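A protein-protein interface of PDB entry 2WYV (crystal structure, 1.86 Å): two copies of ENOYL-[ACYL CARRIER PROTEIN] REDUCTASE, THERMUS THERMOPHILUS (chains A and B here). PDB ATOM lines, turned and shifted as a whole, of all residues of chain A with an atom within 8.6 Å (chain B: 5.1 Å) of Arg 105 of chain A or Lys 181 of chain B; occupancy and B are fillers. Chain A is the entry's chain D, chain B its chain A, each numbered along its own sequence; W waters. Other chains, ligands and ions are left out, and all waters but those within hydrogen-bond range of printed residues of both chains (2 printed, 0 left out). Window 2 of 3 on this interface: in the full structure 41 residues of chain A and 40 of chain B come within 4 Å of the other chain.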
ATOM      1  N   GLU A 100       0.222  11.648 -11.296  1.00  0.00           N
ATOM      2  CA  GLU A 100       1.161  12.565 -10.635  1.00  0.00           C
ATOM      3  C   GLU A 100       2.536  11.894 -10.372  1.00  0.00           C
ATOM      4  O   GLU A 100       3.589  12.550 -10.448  1.00  0.00           O
ATOM      5  CB  GLU A 100       0.552  13.089  -9.324  1.00  0.00           C
ATOM      6  CG  GLU A 100      -0.925  13.599  -9.445  1.00  0.00           C
ATOM      7  CD  GLU A 100      -1.982  12.565  -8.959  1.00  0.00           C
ATOM      8  OE1 GLU A 100      -2.318  12.566  -7.740  1.00  0.00           O
ATOM      9  OE2 GLU A 100      -2.477  11.758  -9.800  1.00  0.00           O
ATOM     10  N   ALA A 101       2.505  10.588 -10.086  1.00  0.00           N
ATOM     11  CA  ALA A 101       3.702   9.795  -9.790  1.00  0.00           C
ATOM     12  C   ALA A 101       4.461   9.386 -11.057  1.00  0.00           C
ATOM     13  O   ALA A 101       5.663   9.088 -10.994  1.00  0.00           O
ATOM     14  CB  ALA A 101       3.319   8.552  -8.977  1.00  0.00           C
ATOM     15  N   MET A 102       3.772   9.374 -12.204  1.00  0.00           N
ATOM     16  CA  MET A 102       4.344   8.847 -13.447  1.00  0.00           C
ATOM     17  C   MET A 102       4.968   9.903 -14.365  1.00  0.00           C
ATOM     18  O   MET A 102       5.548   9.542 -15.393  1.00  0.00           O
ATOM     19  CB  MET A 102       3.289   8.052 -14.244  1.00  0.00           C
ATOM     20  CG  MET A 102       2.752   6.820 -13.531  1.00  0.00           C
ATOM     21  SD  MET A 102       4.073   5.628 -13.256  1.00  0.00           S
ATOM     22  CE  MET A 102       4.298   5.008 -14.924  1.00  0.00           C
ATOM     23  N   GLU A 103       4.804  11.183 -14.026  1.00  0.00           N
ATOM     24  CA  GLU A 103       5.496  12.292 -14.702  1.00  0.00           C
ATOM     25  C   GLU A 103       6.570  12.748 -13.742  1.00  0.00           C
ATOM     26  O   GLU A 103       6.367  12.731 -12.533  1.00  0.00           O
ATOM     27  CB  GLU A 103       4.556  13.480 -14.950  1.00  0.00           C
ATOM     28  CG  GLU A 103       3.347  13.189 -15.830  1.00  0.00           C
ATOM     29  CD  GLU A 103       3.708  12.930 -17.299  1.00  0.00           C
ATOM     30  OE1 GLU A 103       2.804  12.458 -18.042  1.00  0.00           O
ATOM     31  OE2 GLU A 103       4.876  13.193 -17.708  1.00  0.00           O
ATOM     32  N   GLY A 104       7.720  13.140 -14.262  1.00  0.00           N
ATOM     33  CA  GLY A 104       8.753  13.695 -13.395  1.00  0.00           C
ATOM     34  C   GLY A 104       9.603  12.612 -12.779  1.00  0.00           C
ATOM     35  O   GLY A 104       9.878  11.603 -13.428  1.00  0.00           O
ATOM     36  N   ARG A 105      10.028  12.835 -11.535  1.00  0.00           N
ATOM     37  CA  ARG A 105      11.085  12.025 -10.937  1.00  0.00           C
ATOM     38  C   ARG A 105      10.545  11.060  -9.886  1.00  0.00           C
ATOM     39  O   ARG A 105       9.672  11.415  -9.101  1.00  0.00           O
ATOM     40  CB  ARG A 105      12.140  12.940 -10.320  1.00  0.00           C
ATOM     41  CG  ARG A 105      12.673  13.993 -11.271  1.00  0.00           C
ATOM     42  CD  ARG A 105      13.940  14.642 -10.700  1.00  0.00           C
ATOM     43  NE  ARG A 105      13.676  15.247  -9.395  1.00  0.00           N
ATOM     44  CZ  ARG A 105      14.599  15.635  -8.517  1.00  0.00           C
ATOM     45  NH1 ARG A 105      15.903  15.513  -8.766  1.00  0.00           N
ATOM     46  NH2 ARG A 105      14.208  16.151  -7.361  1.00  0.00           N
ATOM     47  N   TYR A 106      11.059   9.834  -9.890  1.00  0.00           N
ATOM     48  CA  TYR A 106      10.741   8.867  -8.843  1.00  0.00           C
ATOM     49  C   TYR A 106      11.019   9.462  -7.443  1.00  0.00           C
ATOM     50  O   TYR A 106      10.245   9.268  -6.521  1.00  0.00           O
ATOM     51  CB  TYR A 106      11.532   7.558  -9.066  1.00  0.00           C
ATOM     52  CG  TYR A 106      11.366   6.537  -7.951  1.00  0.00           C
ATOM     53  CD1 TYR A 106      10.135   5.943  -7.725  1.00  0.00           C
ATOM     54  CD2 TYR A 106      12.440   6.152  -7.149  1.00  0.00           C
ATOM     55  CE1 TYR A 106       9.946   5.005  -6.691  1.00  0.00           C
ATOM     56  CE2 TYR A 106      12.266   5.214  -6.093  1.00  0.00           C
ATOM     57  CZ  TYR A 106      10.994   4.641  -5.890  1.00  0.00           C
ATOM     58  OH  TYR A 106      10.728   3.702  -4.887  1.00  0.00           O
ATOM     59  N   ILE A 107      12.130  10.180  -7.303  1.00  0.00           N
ATOM     60  CA  ILE A 107      12.560  10.735  -6.008  1.00  0.00           C
ATOM     61  C   ILE A 107      11.521  11.683  -5.415  1.00  0.00           C
ATOM     62  O   ILE A 107      11.406  11.796  -4.186  1.00  0.00           O
ATOM     63  CB  ILE A 107      13.939  11.433  -6.091  1.00  0.00           C
ATOM     64  CG1 ILE A 107      14.522  11.652  -4.683  1.00  0.00           C
ATOM     65  CG2 ILE A 107      13.873  12.765  -6.909  1.00  0.00           C
ATOM     66  CD1 ILE A 107      15.972  12.163  -4.686  1.00  0.00           C
ATOM     67  N   ASP A 108      10.762  12.329  -6.300  1.00  0.00           N
ATOM     68  CA  ASP A 108       9.700  13.264  -5.933  1.00  0.00           C
ATOM     69  C   ASP A 108       8.331  12.610  -5.659  1.00  0.00           C
ATOM     70  O   ASP A 108       7.351  13.320  -5.428  1.00  0.00           O
ATOM     71  CB  ASP A 108       9.542  14.325  -7.051  1.00  0.00           C
ATOM     72  CG  ASP A 108      10.725  15.270  -7.146  1.00  0.00           C
ATOM     73  OD1 ASP A 108      10.977  15.811  -8.253  1.00  0.00           O
ATOM     74  OD2 ASP A 108      11.406  15.505  -6.134  1.00  0.00           O
ATOM     75  N   THR A 109       8.230  11.272  -5.668  1.00  0.00           N
ATOM     76  CA  THR A 109       6.935  10.607  -5.402  1.00  0.00           C
ATOM     77  C   THR A 109       6.359  10.827  -3.997  1.00  0.00           C
ATOM     78  O   THR A 109       7.004  10.536  -2.979  1.00  0.00           O
ATOM     79  CB  THR A 109       7.028   9.028  -5.579  1.00  0.00           C
ATOM     80  OG1 THR A 109       7.805   8.723  -6.733  1.00  0.00           O
ATOM     81  CG2 THR A 109       5.642   8.394  -5.659  1.00  0.00           C
ATOM     82  N   ARG A 110       5.103  11.268  -3.956  1.00  0.00           N
ATOM     83  CA  ARG A 110       4.353  11.430  -2.709  1.00  0.00           C
ATOM     84  C   ARG A 110       4.005  10.094  -2.068  1.00  0.00           C
ATOM     85  O   ARG A 110       3.639   9.138  -2.766  1.00  0.00           O
ATOM     86  CB  ARG A 110       3.066  12.232  -2.979  1.00  0.00           C
ATOM     87  CG  ARG A 110       3.334  13.668  -3.447  1.00  0.00           C
ATOM     88  CD  ARG A 110       2.028  14.433  -3.670  1.00  0.00           C
ATOM     89  NE  ARG A 110       1.268  13.961  -4.831  1.00  0.00           N
ATOM     90  CZ  ARG A 110       0.082  14.449  -5.224  1.00  0.00           C
ATOM     91  NH1 ARG A 110      -0.512  15.447  -4.553  1.00  0.00           N
ATOM     92  NH2 ARG A 110      -0.525  13.943  -6.298  1.00  0.00           N
ATOM     93  N   PRO A 155      13.293   5.630 -17.842  1.00  0.00           N
ATOM     94  CA  PRO A 155      12.834   6.925 -17.361  1.00  0.00           C
ATOM     95  C   PRO A 155      11.331   7.101 -17.524  1.00  0.00           C
ATOM     96  O   PRO A 155      10.745   6.508 -18.415  1.00  0.00           O
ATOM     97  CB  PRO A 155      13.614   7.906 -18.243  1.00  0.00           C
ATOM     98  CG  PRO A 155      14.906   7.118 -18.560  1.00  0.00           C
ATOM     99  CD  PRO A 155      14.384   5.771 -18.837  1.00  0.00           C
ATOM    100  N   LYS A 156      10.741   7.891 -16.627  1.00  0.00           N
ATOM    101  CA  LYS A 156       9.283   8.086 -16.492  1.00  0.00           C
ATOM    102  C   LYS A 156       8.459   6.901 -15.929  1.00  0.00           C
ATOM    103  O   LYS A 156       7.346   7.121 -15.457  1.00  0.00           O
ATOM    104  CB  LYS A 156       8.656   8.603 -17.813  1.00  0.00           C
ATOM    105  CG  LYS A 156       9.212   9.963 -18.322  1.00  0.00           C
ATOM    106  CD  LYS A 156       8.133  10.660 -19.185  1.00  0.00           C
ATOM    107  CE  LYS A 156       8.682  11.745 -20.118  1.00  0.00           C
ATOM    108  NZ  LYS A 156       7.612  12.761 -20.456  1.00  0.00           N
ATOM    109  N   TYR A 157       8.962   5.666 -15.947  1.00  0.00           N
ATOM    110  CA  TYR A 157       8.169   4.524 -15.447  1.00  0.00           C
ATOM    111  C   TYR A 157       8.071   4.540 -13.888  1.00  0.00           C
ATOM    112  O   TYR A 157       7.067   4.113 -13.312  1.00  0.00           O
ATOM    113  CB  TYR A 157       8.707   3.194 -15.996  1.00  0.00           C
ATOM    114  CG  TYR A 157       7.721   2.035 -15.965  1.00  0.00           C
ATOM    115  CD1 TYR A 157       6.557   2.054 -16.712  1.00  0.00           C
ATOM    116  CD2 TYR A 157       7.970   0.909 -15.180  1.00  0.00           C
ATOM    117  CE1 TYR A 157       5.640   0.964 -16.676  1.00  0.00           C
ATOM    118  CE2 TYR A 157       7.100  -0.165 -15.142  1.00  0.00           C
ATOM    119  CZ  TYR A 157       5.941  -0.155 -15.894  1.00  0.00           C
ATOM    120  OH  TYR A 157       5.095  -1.250 -15.843  1.00  0.00           O
ATOM    121  N   ASN A 158       9.112   5.071 -13.244  1.00  0.00           N
ATOM    122  CA  ASN A 158       9.071   5.542 -11.849  1.00  0.00           C
ATOM    123  C   ASN A 158       8.546   4.473 -10.885  1.00  0.00           C
ATOM    124  O   ASN A 158       9.002   3.332 -10.964  1.00  0.00           O
ATOM    125  CB  ASN A 158       8.346   6.894 -11.771  1.00  0.00           C
ATOM    126  CG  ASN A 158       9.090   8.009 -12.530  1.00  0.00           C
ATOM    127  OD1 ASN A 158      10.179   7.778 -13.039  1.00  0.00           O
ATOM    128  ND2 ASN A 158       8.506   9.218 -12.590  1.00  0.00           N
ATOM    129  N   VAL A 159       7.567   4.793 -10.045  1.00  0.00           N
ATOM    130  CA  VAL A 159       7.095   3.829  -9.031  1.00  0.00           C
ATOM    131  C   VAL A 159       6.584   2.496  -9.603  1.00  0.00           C
ATOM    132  O   VAL A 159       6.577   1.465  -8.899  1.00  0.00           O
ATOM    133  CB  VAL A 159       6.046   4.447  -8.094  1.00  0.00           C
ATOM    134  CG1 VAL A 159       4.716   4.687  -8.806  1.00  0.00           C
ATOM    135  CG2 VAL A 159       5.813   3.538  -6.903  1.00  0.00           C
ATOM    136  N   GLU B 133      18.663  15.528  -0.828  1.00  0.00           N
ATOM    137  CA  GLU B 133      19.149  16.017  -2.127  1.00  0.00           C
ATOM    138  C   GLU B 133      19.733  17.470  -2.136  1.00  0.00           C
ATOM    139  O   GLU B 133      20.841  17.660  -2.633  1.00  0.00           O
ATOM    140  CB  GLU B 133      18.062  15.896  -3.208  1.00  0.00           C
ATOM    141  CG  GLU B 133      18.529  16.352  -4.601  1.00  0.00           C
ATOM    142  CD  GLU B 133      17.431  16.343  -5.651  1.00  0.00           C
ATOM    143  OE1 GLU B 133      17.784  16.353  -6.845  1.00  0.00           O
ATOM    144  OE2 GLU B 133      16.221  16.337  -5.306  1.00  0.00           O
ATOM    145  N   ARG B 137      26.374  17.306  -1.054  1.00  0.00           N
ATOM    146  CA  ARG B 137      27.436  17.935  -1.825  1.00  0.00           C
ATOM    147  C   ARG B 137      27.942  16.977  -2.919  1.00  0.00           C
ATOM    148  O   ARG B 137      27.822  15.752  -2.801  1.00  0.00           O
ATOM    149  CB  ARG B 137      28.577  18.335  -0.865  1.00  0.00           C
ATOM    150  CG  ARG B 137      28.133  19.217   0.362  1.00  0.00           C
ATOM    151  CD  ARG B 137      29.306  19.405   1.302  1.00  0.00           C
ATOM    152  NE  ARG B 137      29.029  20.220   2.487  1.00  0.00           N
ATOM    153  CZ  ARG B 137      29.201  19.844   3.761  1.00  0.00           C
ATOM    154  NH1 ARG B 137      29.633  18.628   4.085  1.00  0.00           N
ATOM    155  NH2 ARG B 137      28.927  20.704   4.742  1.00  0.00           N
ATOM    156  N   GLU B 138      28.492  17.541  -3.992  1.00  0.00           N
ATOM    157  CA  GLU B 138      29.215  16.758  -5.010  1.00  0.00           C
ATOM    158  C   GLU B 138      30.189  15.780  -4.331  1.00  0.00           C
ATOM    159  O   GLU B 138      30.882  16.131  -3.371  1.00  0.00           O
ATOM    160  CB  GLU B 138      29.955  17.703  -5.992  1.00  0.00           C
ATOM    161  CG  GLU B 138      30.315  17.102  -7.377  1.00  0.00           C
ATOM    162  CD  GLU B 138      31.603  16.285  -7.367  1.00  0.00           C
ATOM    163  OE1 GLU B 138      31.806  15.476  -8.307  1.00  0.00           O
ATOM    164  OE2 GLU B 138      32.418  16.452  -6.425  1.00  0.00           O
ATOM    165  N   GLU B 177      18.715   9.484 -10.907  1.00  0.00           N
ATOM    166  CA  GLU B 177      18.239  10.850 -10.660  1.00  0.00           C
ATOM    167  C   GLU B 177      19.221  11.759  -9.923  1.00  0.00           C
ATOM    168  O   GLU B 177      19.259  12.962 -10.185  1.00  0.00           O
ATOM    169  CB  GLU B 177      16.872  10.790  -9.988  1.00  0.00           C
ATOM    170  CG  GLU B 177      15.845  10.149 -10.906  1.00  0.00           C
ATOM    171  CD  GLU B 177      14.489   9.964 -10.283  1.00  0.00           C
ATOM    172  OE1 GLU B 177      13.534   9.676 -11.028  1.00  0.00           O
ATOM    173  OE2 GLU B 177      14.351  10.120  -9.060  1.00  0.00           O
ATOM    174  N   LEU B 178      20.029  11.198  -9.030  1.00  0.00           N
ATOM    175  CA  LEU B 178      20.995  11.985  -8.245  1.00  0.00           C
ATOM    176  C   LEU B 178      22.368  12.088  -8.923  1.00  0.00           C
ATOM    177  O   LEU B 178      23.176  12.972  -8.591  1.00  0.00           O
ATOM    178  CB  LEU B 178      21.161  11.395  -6.842  1.00  0.00           C
ATOM    179  CG  LEU B 178      19.885  11.462  -5.986  1.00  0.00           C
ATOM    180  CD1 LEU B 178      20.113  10.805  -4.658  1.00  0.00           C
ATOM    181  CD2 LEU B 178      19.394  12.914  -5.789  1.00  0.00           C
ATOM    182  N   GLY B 179      22.631  11.170  -9.847  1.00  0.00           N
ATOM    183  CA  GLY B 179      23.934  11.077 -10.476  1.00  0.00           C
ATOM    184  C   GLY B 179      24.426  12.379 -11.103  1.00  0.00           C
ATOM    185  O   GLY B 179      25.584  12.711 -10.948  1.00  0.00           O
ATOM    186  N   PRO B 180      23.551  13.112 -11.825  1.00  0.00           N
ATOM    187  CA  PRO B 180      23.973  14.373 -12.472  1.00  0.00           C
ATOM    188  C   PRO B 180      24.418  15.495 -11.525  1.00  0.00           C
ATOM    189  O   PRO B 180      25.082  16.432 -11.980  1.00  0.00           O
ATOM    190  CB  PRO B 180      22.726  14.795 -13.253  1.00  0.00           C
ATOM    191  CG  PRO B 180      22.022  13.507 -13.518  1.00  0.00           C
ATOM    192  CD  PRO B 180      22.203  12.724 -12.262  1.00  0.00           C
ATOM    193  N   LYS B 181      24.050  15.395 -10.243  1.00  0.00           N
ATOM    194  CA  LYS B 181      24.523  16.285  -9.170  1.00  0.00           C
ATOM    195  C   LYS B 181      25.835  15.794  -8.592  1.00  0.00           C
ATOM    196  O   LYS B 181      26.389  16.402  -7.692  1.00  0.00           O
ATOM    197  CB  LYS B 181      23.493  16.333  -8.032  1.00  0.00           C
ATOM    198  CG  LYS B 181      22.120  16.816  -8.459  1.00  0.00           C
ATOM    199  CD  LYS B 181      20.970  15.964  -7.898  1.00  0.00           C
ATOM    200  CE  LYS B 181      19.796  15.834  -8.879  1.00  0.00           C
ATOM    201  NZ  LYS B 181      20.232  15.409 -10.256  1.00  0.00           N
ATOM    202  N   GLY B 182      26.317  14.667  -9.095  1.00  0.00           N
ATOM    203  CA  GLY B 182      27.547  14.064  -8.617  1.00  0.00           C
ATOM    204  C   GLY B 182      27.351  13.225  -7.365  1.00  0.00           C
ATOM    205  O   GLY B 182      28.294  13.081  -6.605  1.00  0.00           O
ATOM    206  N   VAL B 183      26.149  12.675  -7.147  1.00  0.00           N
ATOM    207  CA  VAL B 183      25.850  11.868  -5.925  1.00  0.00           C
ATOM    208  C   VAL B 183      25.549  10.383  -6.303  1.00  0.00           C
ATOM    209  O   VAL B 183      24.835  10.130  -7.266  1.00  0.00           O
ATOM    210  CB  VAL B 183      24.677  12.499  -5.109  1.00  0.00           C
ATOM    211  CG1 VAL B 183      24.130  11.518  -3.995  1.00  0.00           C
ATOM    212  CG2 VAL B 183      25.116  13.825  -4.468  1.00  0.00           C
HETATM  213  O   HOH W   1      12.674   8.571 -13.562  1.00  0.00           O
HETATM  214  O   HOH W   2      17.215  14.654 -11.379  1.00  0.00           O
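Water W1 lies within hydrogen-bond range of OD1 of Asn 158 of chain A and OE1 of Glu 177 of chain B. Water W2 lies within hydrogen-bond range of O of Glu 177 of chain B (2.9 Å), NH1 of Arg 105 of chain A (3.0 Å) and NZ of Lys 181 of chain B (3.3 Å).
Among the printed residues, pairs that only touch across the chains: Arg 105 of chain A with Glu 177 of chain B (3.4 Å), Arg 105 of chain A with Lys 181 of chain B (3.9 Å) and Ile 107 of chain A with Leu 178 of chain B (3.7 Å).
The side-chain carboxylate (OE1) of Glu 133 of chain B is in salt-bridge range of the guanidinium group (NH1) of Arg 105 of chain A (2.8 Å). N of Tyr 106 of chain A lies within hydrogen-bond range of OE1 of Glu 177 of chain B, 2.7 Å away. The side-chain carboxylate (OE2) of Glu 177 of chain B lies within hydrogen-bond range of the backbone NH (N) of Ile 107 of chain A (2.8 Å).
Of the printed residues of chain B, Tyr 106 of chain A touches Glu 177 (2.7 Å). Of the printed residues of chain B, Ile 107 of chain A touches Glu 177 (2.8 Å) and Leu 178 (3.7 Å). Printed residues of chain A within 4 Å of Glu 133 of chain B: Arg 105 (2.8 Å). No residue of chain A comes within 4 Å of Gly 179 of chain B. No residue of chain A comes within 4 Å of Gly 182 of chain B. The nearest printed residue of chain B that does not touch Tyr 106 of chain A is Glu 133 of chain B (8.9 Å).
The side-chain amino group (NZ) of Lys 181 of chain B lies within hydrogen-bond range of the backbone carbonyl oxygen (O) of Glu 177 of chain B (2.6 Å). O of Leu 178 of chain B is in hydrogen-bond range of N of Val 183 of chain B, at 3.3 Å. NE of Arg 105 of chain A lies within salt-bridge range of OD1 of Asp 108 of chain A, 3.0 Å away. The backbone carbonyl oxygen of Tyr 106 of chain A sits at hydrogen-bond distance from the side-chain hydroxyl of Thr 109 of chain A.
Printed residues of chain A that touch a printed residue of chain B: Arg 105, Tyr 106 and Ile 107. Of the 10 printed residues of chain B, 4 touch a printed residue of chain A. Printed residues of chain B that touch a printed residue of chain A: Glu 133, Glu 177, Leu 178 and Lys 181. Hydrophobic or aromatic side chains of chain B within 4 Å of the printed part of chain A: Leu 178. Among the printed residues, 6 pairs touch across the chains.
No position is printed for both chains.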
